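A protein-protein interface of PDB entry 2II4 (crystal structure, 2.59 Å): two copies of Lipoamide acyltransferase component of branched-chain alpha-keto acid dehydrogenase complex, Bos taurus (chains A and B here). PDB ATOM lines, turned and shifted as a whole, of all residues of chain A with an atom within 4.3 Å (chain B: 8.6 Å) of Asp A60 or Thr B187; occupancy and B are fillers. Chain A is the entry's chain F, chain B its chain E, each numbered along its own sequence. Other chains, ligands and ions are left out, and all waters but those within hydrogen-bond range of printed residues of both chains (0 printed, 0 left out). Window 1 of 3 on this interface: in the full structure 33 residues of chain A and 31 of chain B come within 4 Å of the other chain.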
ATOM      1  N   TYR A  58      35.678 -17.338  -4.618  1.00  0.00           N
ATOM      2  CA  TYR A  58      34.323 -16.818  -4.646  1.00  0.00           C
ATOM      3  C   TYR A  58      34.424 -15.325  -5.056  1.00  0.00           C
ATOM      4  O   TYR A  58      35.359 -14.593  -4.602  1.00  0.00           O
ATOM      5  CB  TYR A  58      33.670 -17.036  -3.269  1.00  0.00           C
ATOM      6  CG  TYR A  58      32.467 -16.161  -2.946  1.00  0.00           C
ATOM      7  CD1 TYR A  58      32.615 -14.832  -2.628  1.00  0.00           C
ATOM      8  CD2 TYR A  58      31.201 -16.675  -2.939  1.00  0.00           C
ATOM      9  CE1 TYR A  58      31.515 -14.029  -2.328  1.00  0.00           C
ATOM     10  CE2 TYR A  58      30.106 -15.892  -2.645  1.00  0.00           C
ATOM     11  CZ  TYR A  58      30.280 -14.577  -2.357  1.00  0.00           C
ATOM     12  OH  TYR A  58      29.192 -13.774  -2.071  1.00  0.00           O
ATOM     13  N   CYS A  59      33.511 -14.872  -5.914  1.00  0.00           N
ATOM     14  CA  CYS A  59      33.561 -13.503  -6.442  1.00  0.00           C
ATOM     15  C   CYS A  59      32.244 -12.796  -6.294  1.00  0.00           C
ATOM     16  O   CYS A  59      31.164 -13.422  -6.358  1.00  0.00           O
ATOM     17  CB  CYS A  59      33.844 -13.523  -7.934  1.00  0.00           C
ATOM     18  SG  CYS A  59      35.444 -14.161  -8.360  1.00  0.00           S
ATOM     19  N   ASP A  60      32.312 -11.477  -6.192  1.00  0.00           N
ATOM     20  CA  ASP A  60      31.112 -10.709  -6.215  1.00  0.00           C
ATOM     21  C   ASP A  60      31.374  -9.417  -6.872  1.00  0.00           C
ATOM     22  O   ASP A  60      32.523  -9.096  -7.224  1.00  0.00           O
ATOM     23  CB  ASP A  60      30.622 -10.441  -4.787  1.00  0.00           C
ATOM     24  CG  ASP A  60      29.091 -10.269  -4.698  1.00  0.00           C
ATOM     25  OD1 ASP A  60      28.408 -10.093  -5.741  1.00  0.00           O
ATOM     26  OD2 ASP A  60      28.580 -10.355  -3.572  1.00  0.00           O
ATOM     27  N   GLU A  61      30.305  -8.641  -7.008  1.00  0.00           N
ATOM     28  CA  GLU A  61      30.452  -7.275  -7.453  1.00  0.00           C
ATOM     29  C   GLU A  61      29.938  -6.383  -6.360  1.00  0.00           C
ATOM     30  O   GLU A  61      29.024  -6.745  -5.624  1.00  0.00           O
ATOM     31  CB  GLU A  61      29.730  -7.039  -8.792  1.00  0.00           C
ATOM     32  CG  GLU A  61      28.475  -6.180  -8.736  1.00  0.00           C
ATOM     33  CD  GLU A  61      27.829  -5.942 -10.101  1.00  0.00           C
ATOM     34  OE1 GLU A  61      28.225  -6.592 -11.108  1.00  0.00           O
ATOM     35  OE2 GLU A  61      26.898  -5.118 -10.151  1.00  0.00           O
ATOM     36  N   TYR A 188      37.734  -9.525 -12.468  1.00  0.00           N
ATOM     37  CA  TYR A 188      37.954 -10.613 -11.497  1.00  0.00           C
ATOM     38  C   TYR A 188      39.367 -11.152 -11.505  1.00  0.00           C
ATOM     39  O   TYR A 188      40.162 -10.911 -12.423  1.00  0.00           O
ATOM     40  CB  TYR A 188      36.995 -11.763 -11.766  1.00  0.00           C
ATOM     41  CG  TYR A 188      35.534 -11.403 -11.541  1.00  0.00           C
ATOM     42  CD1 TYR A 188      35.067 -11.114 -10.244  1.00  0.00           C
ATOM     43  CD2 TYR A 188      34.598 -11.318 -12.626  1.00  0.00           C
ATOM     44  CE1 TYR A 188      33.708 -10.767 -10.011  1.00  0.00           C
ATOM     45  CE2 TYR A 188      33.197 -10.973 -12.394  1.00  0.00           C
ATOM     46  CZ  TYR A 188      32.786 -10.705 -11.078  1.00  0.00           C
ATOM     47  OH  TYR A 188      31.476 -10.376 -10.737  1.00  0.00           O
ATOM     48  N   ASN A 225      34.685  -5.175  -8.682  1.00  0.00           N
ATOM     49  CA  ASN A 225      34.675  -6.593  -8.501  1.00  0.00           C
ATOM     50  C   ASN A 225      35.624  -6.999  -7.422  1.00  0.00           C
ATOM     51  O   ASN A 225      36.738  -6.470  -7.296  1.00  0.00           O
ATOM     52  CB  ASN A 225      35.072  -7.276  -9.803  1.00  0.00           C
ATOM     53  CG  ASN A 225      34.080  -6.993 -10.926  1.00  0.00           C
ATOM     54  OD1 ASN A 225      34.398  -6.284 -11.883  1.00  0.00           O
ATOM     55  ND2 ASN A 225      32.880  -7.550 -10.811  1.00  0.00           N
ATOM     56  N   VAL A 226      35.175  -7.952  -6.634  1.00  0.00           N
ATOM     57  CA  VAL A 226      36.066  -8.564  -5.696  1.00  0.00           C
ATOM     58  C   VAL A 226      36.161 -10.069  -5.965  1.00  0.00           C
ATOM     59  O   VAL A 226      35.136 -10.730  -6.262  1.00  0.00           O
ATOM     60  CB  VAL A 226      35.615  -8.276  -4.235  1.00  0.00           C
ATOM     61  CG1 VAL A 226      34.253  -8.980  -3.911  1.00  0.00           C
ATOM     62  CG2 VAL A 226      36.729  -8.668  -3.249  1.00  0.00           C
ATOM     63  N   ASN A 245      29.581 -10.697   1.915  1.00  0.00           N
ATOM     64  CA  ASN A 245      28.379  -9.906   2.175  1.00  0.00           C
ATOM     65  C   ASN A 245      28.547  -8.813   3.254  1.00  0.00           C
ATOM     66  O   ASN A 245      28.174  -7.660   3.005  1.00  0.00           O
ATOM     67  CB  ASN A 245      27.195 -10.796   2.456  1.00  0.00           C
ATOM     68  CG  ASN A 245      26.772 -11.591   1.236  1.00  0.00           C
ATOM     69  OD1 ASN A 245      27.202 -11.308   0.105  1.00  0.00           O
ATOM     70  ND2 ASN A 245      25.979 -12.635   1.457  1.00  0.00           N
ATOM     71  N   LYS A 248      31.088  -6.070   1.966  1.00  0.00           N
ATOM     72  CA  LYS A 248      30.327  -5.389   0.967  1.00  0.00           C
ATOM     73  C   LYS A 248      29.332  -4.450   1.636  1.00  0.00           C
ATOM     74  O   LYS A 248      29.247  -3.264   1.300  1.00  0.00           O
ATOM     75  CB  LYS A 248      29.564  -6.461   0.199  1.00  0.00           C
ATOM     76  CG  LYS A 248      29.002  -6.083  -1.127  1.00  0.00           C
ATOM     77  CD  LYS A 248      28.114  -7.244  -1.594  1.00  0.00           C
ATOM     78  CE  LYS A 248      27.320  -6.889  -2.818  1.00  0.00           C
ATOM     79  NZ  LYS A 248      26.482  -8.047  -3.156  1.00  0.00           N
ATOM     80  N   CYS B  59      32.969 -20.413 -17.246  1.00  0.00           N
ATOM     81  CA  CYS B  59      31.891 -19.642 -16.599  1.00  0.00           C
ATOM     82  C   CYS B  59      31.003 -19.061 -17.622  1.00  0.00           C
ATOM     83  O   CYS B  59      31.432 -18.811 -18.717  1.00  0.00           O
ATOM     84  CB  CYS B  59      32.447 -18.462 -15.828  1.00  0.00           C
ATOM     85  SG  CYS B  59      33.605 -18.979 -14.590  1.00  0.00           S
ATOM     86  N   ASP B  60      29.763 -18.791 -17.260  1.00  0.00           N
ATOM     87  CA  ASP B  60      28.883 -18.174 -18.203  1.00  0.00           C
ATOM     88  C   ASP B  60      27.882 -17.310 -17.467  1.00  0.00           C
ATOM     89  O   ASP B  60      27.864 -17.290 -16.234  1.00  0.00           O
ATOM     90  CB  ASP B  60      28.222 -19.244 -19.100  1.00  0.00           C
ATOM     91  CG  ASP B  60      27.897 -18.716 -20.543  1.00  0.00           C
ATOM     92  OD1 ASP B  60      27.939 -17.467 -20.766  1.00  0.00           O
ATOM     93  OD2 ASP B  60      27.601 -19.563 -21.433  1.00  0.00           O
ATOM     94  N   SER B 179      26.589 -26.416  -6.438  1.00  0.00           N
ATOM     95  CA  SER B 179      26.843 -25.628  -5.257  1.00  0.00           C
ATOM     96  C   SER B 179      26.130 -24.339  -5.446  1.00  0.00           C
ATOM     97  O   SER B 179      26.648 -23.408  -6.076  1.00  0.00           O
ATOM     98  CB  SER B 179      28.338 -25.362  -5.128  1.00  0.00           C
ATOM     99  OG  SER B 179      28.643 -24.638  -3.938  1.00  0.00           O
ATOM    100  N   ILE B 181      25.821 -21.524  -4.120  1.00  0.00           N
ATOM    101  CA  ILE B 181      26.311 -20.516  -3.177  1.00  0.00           C
ATOM    102  C   ILE B 181      25.510 -19.220  -3.277  1.00  0.00           C
ATOM    103  O   ILE B 181      25.465 -18.423  -2.334  1.00  0.00           O
ATOM    104  CB  ILE B 181      27.825 -20.286  -3.325  1.00  0.00           C
ATOM    105  CG1 ILE B 181      28.351 -19.389  -2.192  1.00  0.00           C
ATOM    106  CG2 ILE B 181      28.171 -19.713  -4.691  1.00  0.00           C
ATOM    107  CD1 ILE B 181      28.213 -19.993  -0.806  1.00  0.00           C
ATOM    108  N   GLY B 182      24.834 -19.035  -4.416  1.00  0.00           N
ATOM    109  CA  GLY B 182      24.061 -17.832  -4.695  1.00  0.00           C
ATOM    110  C   GLY B 182      22.843 -17.625  -3.805  1.00  0.00           C
ATOM    111  O   GLY B 182      22.267 -16.522  -3.802  1.00  0.00           O
ATOM    112  N   ILE B 184      23.305 -17.581  -0.845  1.00  0.00           N
ATOM    113  CA  ILE B 184      23.893 -16.696   0.131  1.00  0.00           C
ATOM    114  C   ILE B 184      24.391 -15.435  -0.560  1.00  0.00           C
ATOM    115  O   ILE B 184      24.163 -14.335  -0.068  1.00  0.00           O
ATOM    116  CB  ILE B 184      24.989 -17.344   0.978  1.00  0.00           C
ATOM    117  CG1 ILE B 184      24.420 -18.546   1.748  1.00  0.00           C
ATOM    118  CG2 ILE B 184      25.483 -16.355   1.963  1.00  0.00           C
ATOM    119  CD1 ILE B 184      25.468 -19.531   2.367  1.00  0.00           C
ATOM    120  N   GLY B 185      25.033 -15.578  -1.706  1.00  0.00           N
ATOM    121  CA  GLY B 185      25.529 -14.407  -2.414  1.00  0.00           C
ATOM    122  C   GLY B 185      26.443 -14.885  -3.520  1.00  0.00           C
ATOM    123  O   GLY B 185      26.607 -16.108  -3.703  1.00  0.00           O
ATOM    124  N   GLY B 186      26.993 -13.939  -4.274  1.00  0.00           N
ATOM    125  CA  GLY B 186      28.020 -14.203  -5.277  1.00  0.00           C
ATOM    126  C   GLY B 186      27.683 -14.019  -6.756  1.00  0.00           C
ATOM    127  O   GLY B 186      26.526 -13.999  -7.143  1.00  0.00           O
ATOM    128  N   THR B 187      28.723 -13.878  -7.575  1.00  0.00           N
ATOM    129  CA  THR B 187      28.581 -13.922  -9.012  1.00  0.00           C
ATOM    130  C   THR B 187      29.285 -15.182  -9.437  1.00  0.00           C
ATOM    131  O   THR B 187      28.681 -16.256  -9.428  1.00  0.00           O
ATOM    132  CB  THR B 187      29.196 -12.686  -9.701  1.00  0.00           C
ATOM    133  OG1 THR B 187      30.512 -12.440  -9.190  1.00  0.00           O
ATOM    134  CG2 THR B 187      28.316 -11.432  -9.470  1.00  0.00           C
ATOM    135  N   TYR B 188      30.573 -15.074  -9.756  1.00  0.00           N
ATOM    136  CA  TYR B 188      31.350 -16.228 -10.219  1.00  0.00           C
ATOM    137  C   TYR B 188      32.059 -16.852  -9.054  1.00  0.00           C
ATOM    138  O   TYR B 188      32.189 -16.249  -7.986  1.00  0.00           O
ATOM    139  CB  TYR B 188      32.360 -15.830 -11.290  1.00  0.00           C
ATOM    140  CG  TYR B 188      31.732 -15.386 -12.593  1.00  0.00           C
ATOM    141  CD1 TYR B 188      31.080 -16.312 -13.458  1.00  0.00           C
ATOM    142  CD2 TYR B 188      31.767 -14.033 -12.979  1.00  0.00           C
ATOM    143  CE1 TYR B 188      30.471 -15.882 -14.695  1.00  0.00           C
ATOM    144  CE2 TYR B 188      31.178 -13.596 -14.215  1.00  0.00           C
ATOM    145  CZ  TYR B 188      30.530 -14.510 -15.056  1.00  0.00           C
ATOM    146  OH  TYR B 188      29.975 -14.043 -16.254  1.00  0.00           O
ATOM    147  N   ALA B 189      32.544 -18.071  -9.256  1.00  0.00           N
ATOM    148  CA  ALA B 189      33.336 -18.691  -8.213  1.00  0.00           C
ATOM    149  C   ALA B 189      34.341 -19.685  -8.810  1.00  0.00           C
ATOM    150  O   ALA B 189      34.386 -19.896 -10.060  1.00  0.00           O
ATOM    151  CB  ALA B 189      32.414 -19.367  -7.202  1.00  0.00           C
ATOM    152  N   LYS B 190      35.160 -20.273  -7.933  1.00  0.00           N
ATOM    153  CA  LYS B 190      36.041 -21.389  -8.342  1.00  0.00           C
ATOM    154  C   LYS B 190      35.820 -22.508  -7.365  1.00  0.00           C
ATOM    155  O   LYS B 190      36.516 -22.610  -6.350  1.00  0.00           O
ATOM    156  CB  LYS B 190      37.530 -20.997  -8.456  1.00  0.00           C
ATOM    157  CG  LYS B 190      38.480 -22.171  -8.956  1.00  0.00           C
ATOM    158  CD  LYS B 190      39.359 -22.938  -7.807  1.00  0.00           C
ATOM    159  CE  LYS B 190      40.204 -24.063  -8.448  1.00  0.00           C
ATOM    160  NZ  LYS B 190      41.474 -24.589  -7.700  1.00  0.00           N
ATOM    161  N   ALA B 202      29.059 -24.136  -9.759  1.00  0.00           N
ATOM    162  CA  ALA B 202      28.601 -23.217  -8.704  1.00  0.00           C
ATOM    163  C   ALA B 202      27.722 -22.156  -9.297  1.00  0.00           C
ATOM    164  O   ALA B 202      28.079 -21.613 -10.355  1.00  0.00           O
ATOM    165  CB  ALA B 202      29.777 -22.566  -7.929  1.00  0.00           C
ATOM    166  N   LEU B 203      26.595 -21.854  -8.614  1.00  0.00           N
ATOM    167  CA  LEU B 203      25.619 -20.835  -9.057  1.00  0.00           C
ATOM    168  C   LEU B 203      25.659 -19.559  -8.226  1.00  0.00           C
ATOM    169  O   LEU B 203      25.672 -19.606  -7.004  1.00  0.00           O
ATOM    170  CB  LEU B 203      24.215 -21.390  -9.015  1.00  0.00           C
ATOM    171  CG  LEU B 203      23.729 -22.676  -9.716  1.00  0.00           C
ATOM    172  CD1 LEU B 203      24.507 -23.015 -10.951  1.00  0.00           C
ATOM    173  CD2 LEU B 203      23.737 -23.866  -8.785  1.00  0.00           C
ATOM    174  N   GLY B 204      25.697 -18.403  -8.863  1.00  0.00           N
ATOM    175  CA  GLY B 204      25.795 -17.139  -8.119  1.00  0.00           C
ATOM    176  C   GLY B 204      24.399 -16.622  -7.879  1.00  0.00           C
ATOM    177  O   GLY B 204      23.436 -17.301  -8.256  1.00  0.00           O
ATOM    178  N   THR B 205      24.289 -15.455  -7.239  1.00  0.00           N
ATOM    179  CA  THR B 205      22.999 -14.851  -6.980  1.00  0.00           C
ATOM    180  C   THR B 205      22.360 -14.373  -8.256  1.00  0.00           C
ATOM    181  O   THR B 205      23.012 -13.719  -9.079  1.00  0.00           O
ATOM    182  CB  THR B 205      23.094 -13.635  -6.032  1.00  0.00           C
ATOM    183  OG1 THR B 205      23.599 -14.069  -4.774  1.00  0.00           O
ATOM    184  CG2 THR B 205      21.673 -13.006  -5.786  1.00  0.00           C
ATOM    185  N   ILE B 206      21.086 -14.722  -8.403  1.00  0.00           N
ATOM    186  CA  ILE B 206      20.209 -14.225  -9.455  1.00  0.00           C
ATOM    187  C   ILE B 206      19.872 -12.737  -9.223  1.00  0.00           C
ATOM    188  O   ILE B 206      19.296 -12.373  -8.194  1.00  0.00           O
ATOM    189  CB  ILE B 206      18.916 -15.059  -9.492  1.00  0.00           C
ATOM    190  CG1 ILE B 206      19.238 -16.531  -9.743  1.00  0.00           C
ATOM    191  CG2 ILE B 206      17.993 -14.569 -10.553  1.00  0.00           C
ATOM    192  CD1 ILE B 206      18.095 -17.433  -9.334  1.00  0.00           C
ATOM    193  N   LYS B 207      20.227 -11.902 -10.185  1.00  0.00           N
ATOM    194  CA  LYS B 207      20.304 -10.472 -10.006  1.00  0.00           C
ATOM    195  C   LYS B 207      19.766  -9.765 -11.265  1.00  0.00           C
ATOM    196  O   LYS B 207      20.020 -10.175 -12.421  1.00  0.00           O
ATOM    197  CB  LYS B 207      21.779 -10.112  -9.833  1.00  0.00           C
ATOM    198  CG  LYS B 207      22.126  -8.790  -9.177  1.00  0.00           C
ATOM    199  CD  LYS B 207      23.686  -8.757  -8.916  1.00  0.00           C
ATOM    200  CE  LYS B 207      24.064  -8.472  -7.375  1.00  0.00           C
ATOM    201  NZ  LYS B 207      25.535  -8.727  -6.913  1.00  0.00           N
ATOM    202  N   LEU B 209      19.798  -7.208 -14.022  1.00  0.00           N
ATOM    203  CA  LEU B 209      20.798  -6.410 -14.716  1.00  0.00           C
ATOM    204  C   LEU B 209      20.201  -5.884 -16.006  1.00  0.00           C
ATOM    205  O   LEU B 209      19.320  -6.522 -16.570  1.00  0.00           O
ATOM    206  CB  LEU B 209      22.030  -7.258 -15.038  1.00  0.00           C
ATOM    207  CG  LEU B 209      22.914  -7.652 -13.858  1.00  0.00           C
ATOM    208  CD1 LEU B 209      24.147  -8.457 -14.317  1.00  0.00           C
ATOM    209  CD2 LEU B 209      23.339  -6.429 -13.062  1.00  0.00           C
ATOM    210  N   ILE B 223      19.660 -12.183 -14.323  1.00  0.00           N
ATOM    211  CA  ILE B 223      20.935 -12.787 -14.746  1.00  0.00           C
ATOM    212  C   ILE B 223      21.530 -13.599 -13.585  1.00  0.00           C
ATOM    213  O   ILE B 223      21.599 -13.114 -12.444  1.00  0.00           O
ATOM    214  CB  ILE B 223      21.945 -11.696 -15.262  1.00  0.00           C
ATOM    215  CG1 ILE B 223      21.403 -10.954 -16.487  1.00  0.00           C
ATOM    216  CG2 ILE B 223      23.253 -12.295 -15.638  1.00  0.00           C
ATOM    217  CD1 ILE B 223      20.681 -11.796 -17.543  1.00  0.00           C
ATOM    218  N   MET B 224      21.920 -14.841 -13.866  1.00  0.00           N
ATOM    219  CA  MET B 224      22.688 -15.666 -12.931  1.00  0.00           C
ATOM    220  C   MET B 224      24.012 -16.094 -13.555  1.00  0.00           C
ATOM    221  O   MET B 224      24.052 -16.501 -14.726  1.00  0.00           O
ATOM    222  CB  MET B 224      21.913 -16.909 -12.552  1.00  0.00           C
ATOM    223  CG  MET B 224      22.543 -17.733 -11.434  1.00  0.00           C
ATOM    224  SD  MET B 224      21.607 -19.273 -11.130  1.00  0.00           S
ATOM    225  CE  MET B 224      22.190 -20.304 -12.492  1.00  0.00           C
ATOM    226  N   ASN B 225      25.095 -16.015 -12.777  1.00  0.00           N
ATOM    227  CA  ASN B 225      26.373 -16.557 -13.217  1.00  0.00           C
ATOM    228  C   ASN B 225      26.473 -18.039 -12.867  1.00  0.00           C
ATOM    229  O   ASN B 225      25.878 -18.477 -11.901  1.00  0.00           O
ATOM    230  CB  ASN B 225      27.516 -15.721 -12.671  1.00  0.00           C
ATOM    231  CG  ASN B 225      27.426 -14.257 -13.129  1.00  0.00           C
ATOM    232  OD1 ASN B 225      27.211 -13.356 -12.304  1.00  0.00           O
ATOM    233  ND2 ASN B 225      27.561 -14.013 -14.446  1.00  0.00           N
ATOM    234  N   VAL B 226      27.141 -18.820 -13.705  1.00  0.00           N
ATOM    235  CA  VAL B 226      27.482 -20.191 -13.366  1.00  0.00           C
ATOM    236  C   VAL B 226      29.010 -20.362 -13.545  1.00  0.00           C
ATOM    237  O   VAL B 226      29.588 -19.764 -14.459  1.00  0.00           O
ATOM    238  CB  VAL B 226      26.691 -21.225 -14.235  1.00  0.00           C
ATOM    239  CG1 VAL B 226      27.115 -21.168 -15.649  1.00  0.00           C
ATOM    240  CG2 VAL B 226      26.915 -22.616 -13.734  1.00  0.00           C
ATOM    241  N   SER B 227      29.642 -21.160 -12.676  1.00  0.00           N
ATOM    242  CA  SER B 227      31.067 -21.485 -12.749  1.00  0.00           C
ATOM    243  C   SER B 227      31.251 -23.001 -12.691  1.00  0.00           C
ATOM    244  O   SER B 227      30.803 -23.640 -11.726  1.00  0.00           O
ATOM    245  CB  SER B 227      31.825 -20.813 -11.625  1.00  0.00           C
ATOM    246  OG  SER B 227      31.654 -19.403 -11.729  1.00  0.00           O
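The side-chain amide nitrogen (ND2) of Asn A245 lies within hydrogen-bond range of the backbone carbonyl oxygen (O) of Ile B184 (2.9 Å). OG1 of Thr B187 is in hydrogen-bond range of OH of Tyr A188 (2.8 Å). OH of Tyr A58 is in hydrogen-bond range of N of Gly B186, at 3.1 Å. The backbone carbonyl oxygen (O) of Tyr B188 is in hydrogen-bond range of the backbone NH (N) of Cys A59 (2.8 Å). The backbone NH (N) of Thr B187 lies within hydrogen-bond range of the backbone carbonyl oxygen (O) of Cys A59 (2.8 Å). NZ of Lys B207 lies within salt-bridge range of OD1 of Asp A60, at 3.4 Å.
The backbone carbonyl oxygen (O) of Lys B207 is in hydrogen-bond range of the backbone NH (N) of Ile B223 (2.8 Å). N of Thr B205 is in hydrogen-bond range of O of Gly B186, at 2.7 Å. The backbone carbonyl oxygen (O) of Val A226 sits at hydrogen-bond distance from the backbone NH (N) of Asp A60 (2.9 Å). The side-chain hydroxyl (OH) of Tyr B188 is in hydrogen-bond range of the side-chain amide nitrogen (ND2) of Asn B225 (3.0 Å). The side-chain amino group (NZ) of Lys A248 lies within salt-bridge range of the side-chain carboxylate (OD2) of Asp A60 (3.1 Å). The side-chain hydroxyl (OH) of Tyr A188 is in hydrogen-bond range of the side-chain amide nitrogen (ND2) of Asn A225, 3.2 Å away.
Ile B181 touches Tyr A58 (CG1 to CE2, 3.9 Å). C of Gly B185 touches OH of Tyr A58, at 3.3 Å. Tyr B188 touches Tyr A58. O of Cys A59 touches CA of Gly B186, at 3.4 Å. OD2 of Asp A60 touches N of Gly B186, 3.98 Å away. OG1 of Thr B187 touches CA of Asp A60, 3.5 Å away. Tyr B188 touches Tyr A188 (CD2 to CE2, 3.4 Å). Lys B207 touches Lys A248.
Of the printed residues of chain B, Cys A59 touches Gly B186 (3.4 Å), Thr B187 (2.8 Å) and Tyr B188 (2.8 Å). Printed residues of chain B within 4 Å of Asp A60: Gly B186 (3.98 Å), Thr B187 (3.5 Å) and Lys B207 (3.4 Å). Of the printed residues of chain B, Tyr A188 touches Thr B187 and Tyr B188. Of the printed residues of chain B, Asn A245 touches Ile B184. Gly B182 touches none of the printed residues of chain A. Of the printed residues of chain A, Gly B185 touches Tyr A58 (3.3 Å). Of the printed residues of chain A, Gly B186 touches Tyr A58, Cys A59 and Asp A60. Of chain A, only Cys A59, Asp A60 and Tyr A188 come within 4 Å of Thr B187.
Hydrophobic or aromatic side chains of chain A within 4 Å of the printed part of chain B: Tyr A58 and Tyr A188. Among the printed residues, 14 pairs touch across the chains.
Cys A59 touches Tyr B188, but with the chains exchanged Tyr A188 does not touch Cys B59 (8.0 Å). Tyr A188 touches its own counterpart, Tyr B188. Positions printed for both chains: 59, 60, 188, 225 and 226. Of the 14 pairs that touch across the chains among the printed residues, 1 has its exchanged pair printed and touching as well.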
